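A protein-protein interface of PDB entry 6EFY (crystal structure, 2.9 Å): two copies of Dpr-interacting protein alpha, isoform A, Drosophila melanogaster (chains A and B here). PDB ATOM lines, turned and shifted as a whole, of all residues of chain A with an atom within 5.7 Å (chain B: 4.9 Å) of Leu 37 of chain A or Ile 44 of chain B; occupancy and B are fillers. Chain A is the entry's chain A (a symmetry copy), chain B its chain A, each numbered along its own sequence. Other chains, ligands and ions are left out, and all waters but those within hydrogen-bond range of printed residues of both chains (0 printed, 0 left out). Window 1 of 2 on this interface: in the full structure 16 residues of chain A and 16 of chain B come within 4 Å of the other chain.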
ATOM      1  N   GLY A  35     -16.729   7.095 -17.848  1.00  0.00           N
ATOM      2  CA  GLY A  35     -16.056   7.679 -18.984  1.00  0.00           C
ATOM      3  C   GLY A  35     -16.103   6.759 -20.188  1.00  0.00           C
ATOM      4  O   GLY A  35     -16.238   5.542 -20.071  1.00  0.00           O
ATOM      5  N   TRP A  36     -15.980   7.371 -21.361  1.00  0.00           N
ATOM      6  CA  TRP A  36     -15.998   6.660 -22.631  1.00  0.00           C
ATOM      7  C   TRP A  36     -14.682   6.882 -23.357  1.00  0.00           C
ATOM      8  O   TRP A  36     -14.111   7.975 -23.300  1.00  0.00           O
ATOM      9  CB  TRP A  36     -17.149   7.136 -23.525  1.00  0.00           C
ATOM     10  CG  TRP A  36     -18.513   6.895 -22.971  1.00  0.00           C
ATOM     11  CD1 TRP A  36     -19.227   7.726 -22.156  1.00  0.00           C
ATOM     12  CD2 TRP A  36     -19.344   5.754 -23.208  1.00  0.00           C
ATOM     13  NE1 TRP A  36     -20.449   7.168 -21.864  1.00  0.00           N
ATOM     14  CE2 TRP A  36     -20.544   5.956 -22.498  1.00  0.00           C
ATOM     15  CE3 TRP A  36     -19.187   4.578 -23.946  1.00  0.00           C
ATOM     16  CZ2 TRP A  36     -21.580   5.026 -22.506  1.00  0.00           C
ATOM     17  CZ3 TRP A  36     -20.220   3.655 -23.954  1.00  0.00           C
ATOM     18  CH2 TRP A  36     -21.400   3.885 -23.239  1.00  0.00           C
ATOM     19  N   LEU A  37     -14.204   5.850 -24.049  1.00  0.00           N
ATOM     20  CA  LEU A  37     -13.100   6.044 -24.975  1.00  0.00           C
ATOM     21  C   LEU A  37     -13.229   5.070 -26.135  1.00  0.00           C
ATOM     22  O   LEU A  37     -13.678   3.932 -25.961  1.00  0.00           O
ATOM     23  CB  LEU A  37     -11.736   5.899 -24.280  1.00  0.00           C
ATOM     24  CG  LEU A  37     -11.143   4.577 -23.795  1.00  0.00           C
ATOM     25  CD1 LEU A  37     -10.367   3.858 -24.888  1.00  0.00           C
ATOM     26  CD2 LEU A  37     -10.234   4.852 -22.613  1.00  0.00           C
ATOM     27  N   LYS A  38     -12.845   5.537 -27.322  1.00  0.00           N
ATOM     28  CA  LYS A  38     -12.850   4.700 -28.514  1.00  0.00           C
ATOM     29  C   LYS A  38     -11.833   3.575 -28.358  1.00  0.00           C
ATOM     30  O   LYS A  38     -10.650   3.826 -28.117  1.00  0.00           O
ATOM     31  CB  LYS A  38     -12.539   5.551 -29.745  1.00  0.00           C
ATOM     32  CG  LYS A  38     -12.582   4.809 -31.071  1.00  0.00           C
ATOM     33  CD  LYS A  38     -14.000   4.424 -31.461  1.00  0.00           C
ATOM     34  CE  LYS A  38     -14.009   3.526 -32.688  1.00  0.00           C
ATOM     35  NZ  LYS A  38     -13.184   4.088 -33.796  1.00  0.00           N
ATOM     36  N   ALA A  39     -12.292   2.332 -28.508  1.00  0.00           N
ATOM     37  CA  ALA A  39     -11.473   1.183 -28.133  1.00  0.00           C
ATOM     38  C   ALA A  39     -10.225   1.054 -29.003  1.00  0.00           C
ATOM     39  O   ALA A  39      -9.123   0.847 -28.484  1.00  0.00           O
ATOM     40  CB  ALA A  39     -12.302  -0.098 -28.198  1.00  0.00           C
ATOM     41  N   LYS A  42      -7.942   4.020 -28.779  1.00  0.00           N
ATOM     42  CA  LYS A  42      -7.719   4.287 -27.360  1.00  0.00           C
ATOM     43  C   LYS A  42      -7.919   5.759 -27.021  1.00  0.00           C
ATOM     44  O   LYS A  42      -7.454   6.233 -25.979  1.00  0.00           O
ATOM     45  CB  LYS A  42      -6.336   3.799 -26.910  1.00  0.00           C
ATOM     46  CG  LYS A  42      -6.079   2.335 -27.247  1.00  0.00           C
ATOM     47  CD  LYS A  42      -4.752   1.845 -26.703  1.00  0.00           C
ATOM     48  CE  LYS A  42      -4.485   0.412 -27.144  1.00  0.00           C
ATOM     49  NZ  LYS A  42      -3.201  -0.127 -26.605  1.00  0.00           N
ATOM     50  N   ALA A  43      -8.626   6.487 -27.882  1.00  0.00           N
ATOM     51  CA  ALA A  43      -8.843   7.915 -27.697  1.00  0.00           C
ATOM     52  C   ALA A  43      -9.959   8.145 -26.690  1.00  0.00           C
ATOM     53  O   ALA A  43     -11.073   7.640 -26.862  1.00  0.00           O
ATOM     54  CB  ALA A  43      -9.182   8.577 -29.030  1.00  0.00           C
ATOM     55  N   ILE A  44      -9.659   8.916 -25.645  1.00  0.00           N
ATOM     56  CA  ILE A  44     -10.657   9.249 -24.638  1.00  0.00           C
ATOM     57  C   ILE A  44     -11.754  10.080 -25.282  1.00  0.00           C
ATOM     58  O   ILE A  44     -11.498  11.165 -25.817  1.00  0.00           O
ATOM     59  CB  ILE A  44     -10.011   9.997 -23.468  1.00  0.00           C
ATOM     60  CG1 ILE A  44      -8.943   9.128 -22.805  1.00  0.00           C
ATOM     61  CG2 ILE A  44     -11.067  10.424 -22.461  1.00  0.00           C
ATOM     62  CD1 ILE A  44      -8.100   9.870 -21.800  1.00  0.00           C
ATOM     63  N   GLN A  45     -12.985   9.574 -25.236  1.00  0.00           N
ATOM     64  CA  GLN A  45     -14.117  10.332 -25.754  1.00  0.00           C
ATOM     65  C   GLN A  45     -14.687  11.280 -24.704  1.00  0.00           C
ATOM     66  O   GLN A  45     -14.836  12.480 -24.962  1.00  0.00           O
ATOM     67  CB  GLN A  45     -15.207   9.383 -26.262  1.00  0.00           C
ATOM     68  CG  GLN A  45     -14.759   8.478 -27.399  1.00  0.00           C
ATOM     69  CD  GLN A  45     -14.197   9.251 -28.578  1.00  0.00           C
ATOM     70  OE1 GLN A  45     -14.936   9.896 -29.322  1.00  0.00           O
ATOM     71  NE2 GLN A  45     -12.881   9.186 -28.757  1.00  0.00           N
ATOM     72  N   ALA A  46     -14.992  10.771 -23.512  1.00  0.00           N
ATOM     73  CA  ALA A  46     -15.626  11.596 -22.496  1.00  0.00           C
ATOM     74  C   ALA A  46     -15.370  11.010 -21.116  1.00  0.00           C
ATOM     75  O   ALA A  46     -14.957   9.857 -20.977  1.00  0.00           O
ATOM     76  CB  ALA A  46     -17.129  11.715 -22.744  1.00  0.00           C
ATOM     77  N   ILE A  47     -15.633  11.827 -20.097  1.00  0.00           N
ATOM     78  CA  ILE A  47     -15.668  11.377 -18.706  1.00  0.00           C
ATOM     79  C   ILE A  47     -16.814  12.112 -18.015  1.00  0.00           C
ATOM     80  O   ILE A  47     -16.889  13.343 -18.082  1.00  0.00           O
ATOM     81  CB  ILE A  47     -14.330  11.622 -17.974  1.00  0.00           C
ATOM     82  CG1 ILE A  47     -14.420  11.159 -16.521  1.00  0.00           C
ATOM     83  CG2 ILE A  47     -13.893  13.087 -18.050  1.00  0.00           C
ATOM     84  CD1 ILE A  47     -14.442   9.653 -16.365  1.00  0.00           C
ATOM     85  N   GLY A  82     -14.934  -0.172 -31.434  1.00  0.00           N
ATOM     86  CA  GLY A  82     -15.391  -0.351 -30.075  1.00  0.00           C
ATOM     87  C   GLY A  82     -15.624   0.960 -29.351  1.00  0.00           C
ATOM     88  O   GLY A  82     -14.985   1.971 -29.626  1.00  0.00           O
ATOM     89  N   TYR A  83     -16.577   0.927 -28.425  1.00  0.00           N
ATOM     90  CA  TYR A  83     -16.856   2.049 -27.539  1.00  0.00           C
ATOM     91  C   TYR A  83     -16.978   1.509 -26.125  1.00  0.00           C
ATOM     92  O   TYR A  83     -17.879   0.715 -25.836  1.00  0.00           O
ATOM     93  CB  TYR A  83     -18.118   2.799 -27.977  1.00  0.00           C
ATOM     94  CG  TYR A  83     -17.870   3.597 -29.236  1.00  0.00           C
ATOM     95  CD1 TYR A  83     -17.981   3.009 -30.491  1.00  0.00           C
ATOM     96  CD2 TYR A  83     -17.481   4.927 -29.168  1.00  0.00           C
ATOM     97  CE1 TYR A  83     -17.730   3.732 -31.643  1.00  0.00           C
ATOM     98  CE2 TYR A  83     -17.231   5.659 -30.313  1.00  0.00           C
ATOM     99  CZ  TYR A  83     -17.356   5.060 -31.546  1.00  0.00           C
ATOM    100  OH  TYR A  83     -17.095   5.801 -32.675  1.00  0.00           O
ATOM    101  N   MET A  84     -16.058   1.920 -25.260  1.00  0.00           N
ATOM    102  CA  MET A  84     -15.921   1.371 -23.920  1.00  0.00           C
ATOM    103  C   MET A  84     -16.320   2.427 -22.903  1.00  0.00           C
ATOM    104  O   MET A  84     -15.742   3.519 -22.879  1.00  0.00           O
ATOM    105  CB  MET A  84     -14.486   0.901 -23.676  1.00  0.00           C
ATOM    106  CG  MET A  84     -14.190   0.466 -22.245  1.00  0.00           C
ATOM    107  SD  MET A  84     -12.492  -0.115 -22.011  1.00  0.00           S
ATOM    108  CE  MET A  84     -11.575   1.367 -22.390  1.00  0.00           C
ATOM    109  N   CYS A  85     -17.315   2.110 -22.080  1.00  0.00           N
ATOM    110  CA  CYS A  85     -17.595   2.878 -20.879  1.00  0.00           C
ATOM    111  C   CYS A  85     -16.932   2.180 -19.705  1.00  0.00           C
ATOM    112  O   CYS A  85     -16.965   0.950 -19.598  1.00  0.00           O
ATOM    113  CB  CYS A  85     -19.094   3.030 -20.621  1.00  0.00           C
ATOM    114  SG  CYS A  85     -19.863   1.622 -19.796  1.00  0.00           S
ATOM    115  N   GLN A  86     -16.312   2.966 -18.836  1.00  0.00           N
ATOM    116  CA  GLN A  86     -15.549   2.416 -17.731  1.00  0.00           C
ATOM    117  C   GLN A  86     -15.800   3.246 -16.486  1.00  0.00           C
ATOM    118  O   GLN A  86     -15.903   4.475 -16.556  1.00  0.00           O
ATOM    119  CB  GLN A  86     -14.048   2.383 -18.054  1.00  0.00           C
ATOM    120  CG  GLN A  86     -13.488   3.723 -18.517  1.00  0.00           C
ATOM    121  CD  GLN A  86     -11.973   3.736 -18.593  1.00  0.00           C
ATOM    122  OE1 GLN A  86     -11.297   4.091 -17.626  1.00  0.00           O
ATOM    123  NE2 GLN A  86     -11.434   3.355 -19.743  1.00  0.00           N
ATOM    124  N   ASN A  88     -14.190   4.500 -12.975  1.00  0.00           N
ATOM    125  CA  ASN A  88     -12.835   4.730 -12.477  1.00  0.00           C
ATOM    126  C   ASN A  88     -12.583   4.083 -11.118  1.00  0.00           C
ATOM    127  O   ASN A  88     -11.892   4.659 -10.273  1.00  0.00           O
ATOM    128  CB  ASN A  88     -12.557   6.230 -12.432  1.00  0.00           C
ATOM    129  CG  ASN A  88     -13.508   6.974 -11.522  1.00  0.00           C
ATOM    130  OD1 ASN A  88     -14.492   6.414 -11.043  1.00  0.00           O
ATOM    131  ND2 ASN A  88     -13.226   8.253 -11.287  1.00  0.00           N
ATOM    132  N   MET A  92     -10.320  -0.749 -12.450  1.00  0.00           N
ATOM    133  CA  MET A  92     -11.482  -0.255 -13.171  1.00  0.00           C
ATOM    134  C   MET A  92     -12.258  -1.402 -13.803  1.00  0.00           C
ATOM    135  O   MET A  92     -11.695  -2.438 -14.173  1.00  0.00           O
ATOM    136  CB  MET A  92     -11.068   0.755 -14.244  1.00  0.00           C
ATOM    137  CG  MET A  92     -10.443   0.158 -15.494  1.00  0.00           C
ATOM    138  SD  MET A  92     -11.632  -0.205 -16.799  1.00  0.00           S
ATOM    139  CE  MET A  92     -10.756   0.381 -18.241  1.00  0.00           C
ATOM    140  N   TRP B  36      -3.769  10.985 -19.641  1.00  0.00           N
ATOM    141  CA  TRP B  36      -3.014   9.748 -19.510  1.00  0.00           C
ATOM    142  C   TRP B  36      -3.973   8.583 -19.334  1.00  0.00           C
ATOM    143  O   TRP B  36      -5.008   8.716 -18.674  1.00  0.00           O
ATOM    144  CB  TRP B  36      -2.061   9.796 -18.309  1.00  0.00           C
ATOM    145  CG  TRP B  36      -1.002  10.844 -18.391  1.00  0.00           C
ATOM    146  CD1 TRP B  36      -1.092  12.138 -17.964  1.00  0.00           C
ATOM    147  CD2 TRP B  36       0.320  10.685 -18.914  1.00  0.00           C
ATOM    148  NE1 TRP B  36       0.091  12.796 -18.198  1.00  0.00           N
ATOM    149  CE2 TRP B  36       0.974  11.926 -18.781  1.00  0.00           C
ATOM    150  CE3 TRP B  36       1.013   9.615 -19.488  1.00  0.00           C
ATOM    151  CZ2 TRP B  36       2.287  12.125 -19.200  1.00  0.00           C
ATOM    152  CZ3 TRP B  36       2.319   9.815 -19.903  1.00  0.00           C
ATOM    153  CH2 TRP B  36       2.942  11.060 -19.756  1.00  0.00           C
ATOM    154  N   LEU B  37      -3.627   7.436 -19.915  1.00  0.00           N
ATOM    155  CA  LEU B  37      -4.342   6.212 -19.591  1.00  0.00           C
ATOM    156  C   LEU B  37      -3.395   5.026 -19.693  1.00  0.00           C
ATOM    157  O   LEU B  37      -2.505   4.998 -20.549  1.00  0.00           O
ATOM    158  CB  LEU B  37      -5.575   6.014 -20.487  1.00  0.00           C
ATOM    159  CG  LEU B  37      -5.525   5.634 -21.967  1.00  0.00           C
ATOM    160  CD1 LEU B  37      -5.459   4.128 -22.173  1.00  0.00           C
ATOM    161  CD2 LEU B  37      -6.750   6.196 -22.659  1.00  0.00           C
ATOM    162  N   LYS B  42      -6.340  -0.115 -20.666  1.00  0.00           N
ATOM    163  CA  LYS B  42      -7.078   0.982 -21.290  1.00  0.00           C
ATOM    164  C   LYS B  42      -7.769   1.862 -20.254  1.00  0.00           C
ATOM    165  O   LYS B  42      -8.696   2.609 -20.582  1.00  0.00           O
ATOM    166  CB  LYS B  42      -8.080   0.461 -22.329  1.00  0.00           C
ATOM    167  CG  LYS B  42      -7.441  -0.443 -23.376  1.00  0.00           C
ATOM    168  CD  LYS B  42      -8.424  -0.862 -24.451  1.00  0.00           C
ATOM    169  CE  LYS B  42      -7.778  -1.842 -25.420  1.00  0.00           C
ATOM    170  NZ  LYS B  42      -8.701  -2.258 -26.517  1.00  0.00           N
ATOM    171  N   ALA B  43      -7.313   1.797 -19.005  1.00  0.00           N
ATOM    172  CA  ALA B  43      -7.920   2.548 -17.916  1.00  0.00           C
ATOM    173  C   ALA B  43      -7.436   3.990 -17.947  1.00  0.00           C
ATOM    174  O   ALA B  43      -6.228   4.247 -17.920  1.00  0.00           O
ATOM    175  CB  ALA B  43      -7.587   1.902 -16.575  1.00  0.00           C
ATOM    176  N   ILE B  44      -8.383   4.927 -17.993  1.00  0.00           N
ATOM    177  CA  ILE B  44      -8.047   6.345 -17.977  1.00  0.00           C
ATOM    178  C   ILE B  44      -7.393   6.685 -16.649  1.00  0.00           C
ATOM    179  O   ILE B  44      -7.994   6.511 -15.582  1.00  0.00           O
ATOM    180  CB  ILE B  44      -9.298   7.196 -18.213  1.00  0.00           C
ATOM    181  CG1 ILE B  44      -9.914   6.871 -19.574  1.00  0.00           C
ATOM    182  CG2 ILE B  44      -8.963   8.675 -18.106  1.00  0.00           C
ATOM    183  CD1 ILE B  44     -11.272   7.491 -19.783  1.00  0.00           C
ATOM    184  N   GLN B  45      -6.155   7.173 -16.706  1.00  0.00           N
ATOM    185  CA  GLN B  45      -5.474   7.606 -15.492  1.00  0.00           C
ATOM    186  C   GLN B  45      -5.810   9.052 -15.143  1.00  0.00           C
ATOM    187  O   GLN B  45      -6.224   9.341 -14.015  1.00  0.00           O
ATOM    188  CB  GLN B  45      -3.958   7.431 -15.640  1.00  0.00           C
ATOM    189  CG  GLN B  45      -3.521   5.994 -15.873  1.00  0.00           C
ATOM    190  CD  GLN B  45      -4.017   5.047 -14.795  1.00  0.00           C
ATOM    191  OE1 GLN B  45      -3.528   5.063 -13.665  1.00  0.00           O
ATOM    192  NE2 GLN B  45      -4.993   4.214 -15.141  1.00  0.00           N
ATOM    193  N   ALA B  46      -5.659   9.969 -16.097  1.00  0.00           N
ATOM    194  CA  ALA B  46      -5.870  11.379 -15.807  1.00  0.00           C
ATOM    195  C   ALA B  46      -6.189  12.131 -17.089  1.00  0.00           C
ATOM    196  O   ALA B  46      -5.976  11.629 -18.195  1.00  0.00           O
ATOM    197  CB  ALA B  46      -4.644  11.990 -15.132  1.00  0.00           C
ATOM    198  N   ILE B  52      -8.339  10.617 -12.524  1.00  0.00           N
ATOM    199  CA  ILE B  52      -9.557   9.838 -12.718  1.00  0.00           C
ATOM    200  C   ILE B  52      -9.491   8.506 -11.987  1.00  0.00           C
ATOM    201  O   ILE B  52     -10.425   8.136 -11.276  1.00  0.00           O
ATOM    202  CB  ILE B  52      -9.841   9.645 -14.225  1.00  0.00           C
ATOM    203  CG1 ILE B  52     -10.390  10.934 -14.841  1.00  0.00           C
ATOM    204  CG2 ILE B  52     -10.827   8.516 -14.450  1.00  0.00           C
ATOM    205  CD1 ILE B  52      -9.344  11.976 -15.146  1.00  0.00           C
ATOM    206  N   THR B  53      -8.391   7.775 -12.139  1.00  0.00           N
ATOM    207  CA  THR B  53      -8.273   6.480 -11.484  1.00  0.00           C
ATOM    208  C   THR B  53      -8.186   6.654  -9.975  1.00  0.00           C
ATOM    209  O   THR B  53      -7.606   7.622  -9.475  1.00  0.00           O
ATOM    210  CB  THR B  53      -7.047   5.727 -11.994  1.00  0.00           C
ATOM    211  OG1 THR B  53      -6.959   4.461 -11.330  1.00  0.00           O
ATOM    212  CG2 THR B  53      -5.783   6.523 -11.734  1.00  0.00           C
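The side-chain amide nitrogen of Gln 45 of chain B is in hydrogen-bond range of the backbone carbonyl oxygen of Ala 43 of chain B (3.0 Å). N of Ile 52 of chain B sits at hydrogen-bond distance from O of Gln 45 of chain B. The backbone NH (N) of Gln 86 of chain A sits at hydrogen-bond distance from the backbone carbonyl oxygen (O) of Gly 35 of chain A (2.9 Å). The backbone carbonyl oxygen of Met 84 of chain A lies within hydrogen-bond range of the backbone NH of Leu 37 of chain A (3.0 Å). N of Ala 39 of chain A sits at hydrogen-bond distance from O of Gly 82 of chain A (2.9 Å).
Hydrophobic or aromatic side chains of chain A within 4 Å of the printed part of chain B: Leu 37, Ile 44, Met 84 and Met 92. Along chain A the printed residues that touch a printed residue of chain B span positions 37 to 92. Of the 9 printed residues of chain B, 5 touch a printed residue of chain A. Along chain B the printed residues that touch a printed residue of chain A span positions 37 to 52.
The backbone carbonyl oxygen of Lys 42 of chain B is in hydrogen-bond range of the side-chain amide nitrogen of Gln 86 of chain A, at 3.0 Å. The backbone NH (N) of Ile 44 of chain B lies within hydrogen-bond range of the side-chain amide oxygen (OE1) of Gln 86 of chain A (3.1 Å). The backbone carbonyl oxygen of Ile 52 of chain B is in hydrogen-bond range of the side-chain amide nitrogen of Asn 88 of chain A (2.8 Å).
Printed residues of chain B within 4 Å of Leu 37 of chain A: Leu 37, Lys 42 and Ile 44. Lys 38 of chain A touches none of the printed residues of chain B. Of the printed residues of chain B, Ala 39 of chain A touches Lys 42. Of the printed residues of chain B, Lys 42 of chain A touches Leu 37 (3.4 Å). Gly 82 of chain A touches none of the printed residues of chain B. Of the printed residues of chain B, Gln 86 of chain A touches Lys 42, Ala 43 and Ile 44. Of the printed residues of chain A, Ile 44 of chain B touches Leu 37, Ile 44 and Gln 86. The nearest printed residue of chain A that does not touch Ile 44 of chain B is Ala 46 of chain A (4.5 Å). The nearest printed residue of chain A that does not touch Leu 37 of chain B is Ala 43 of chain A (5.5 Å).
CD2 of Leu 37 of chain A touches CD2 of Leu 37 of chain B, at 3.7 Å. Leu 37 of chain A touches Lys 42 of chain B (CD2 to O, 3.4 Å). Leu 37 of chain A touches Ile 44 of chain B. Ala 39 of chain A touches Lys 42 of chain B. Lys 42 of chain A touches Leu 37 of chain B. Ile 44 of chain A touches Ile 44 of chain B. Met 84 of chain A touches Lys 42 of chain B (CE to CB, 3.6 Å). Ala 43 of chain B touches Gln 86 of chain A (CA to OE1, 3.7 Å). Met 92 of chain A touches Lys 42 of chain B (CE to O, 3.8 Å). Met 92 of chain A touches Ala 43 of chain B.
Leu 37 of chain B touches its own counterpart, Leu 37 of chain A. Leu 37 of chain A touches Lys 42 of chain B, and with the chains exchanged Lys 42 of chain A touches Leu 37 of chain B. Leu 37 of chain A touches Ile 44 of chain B, and with the chains exchanged Ile 44 of chain A touches Leu 37 of chain B. Ile 44 of chain B touches its own counterpart, Ile 44 of chain A. 7 positions are printed for both chains. Of the 14 pairs that touch across the chains among the printed residues, 6 have their exchanged pair printed and touching as well.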
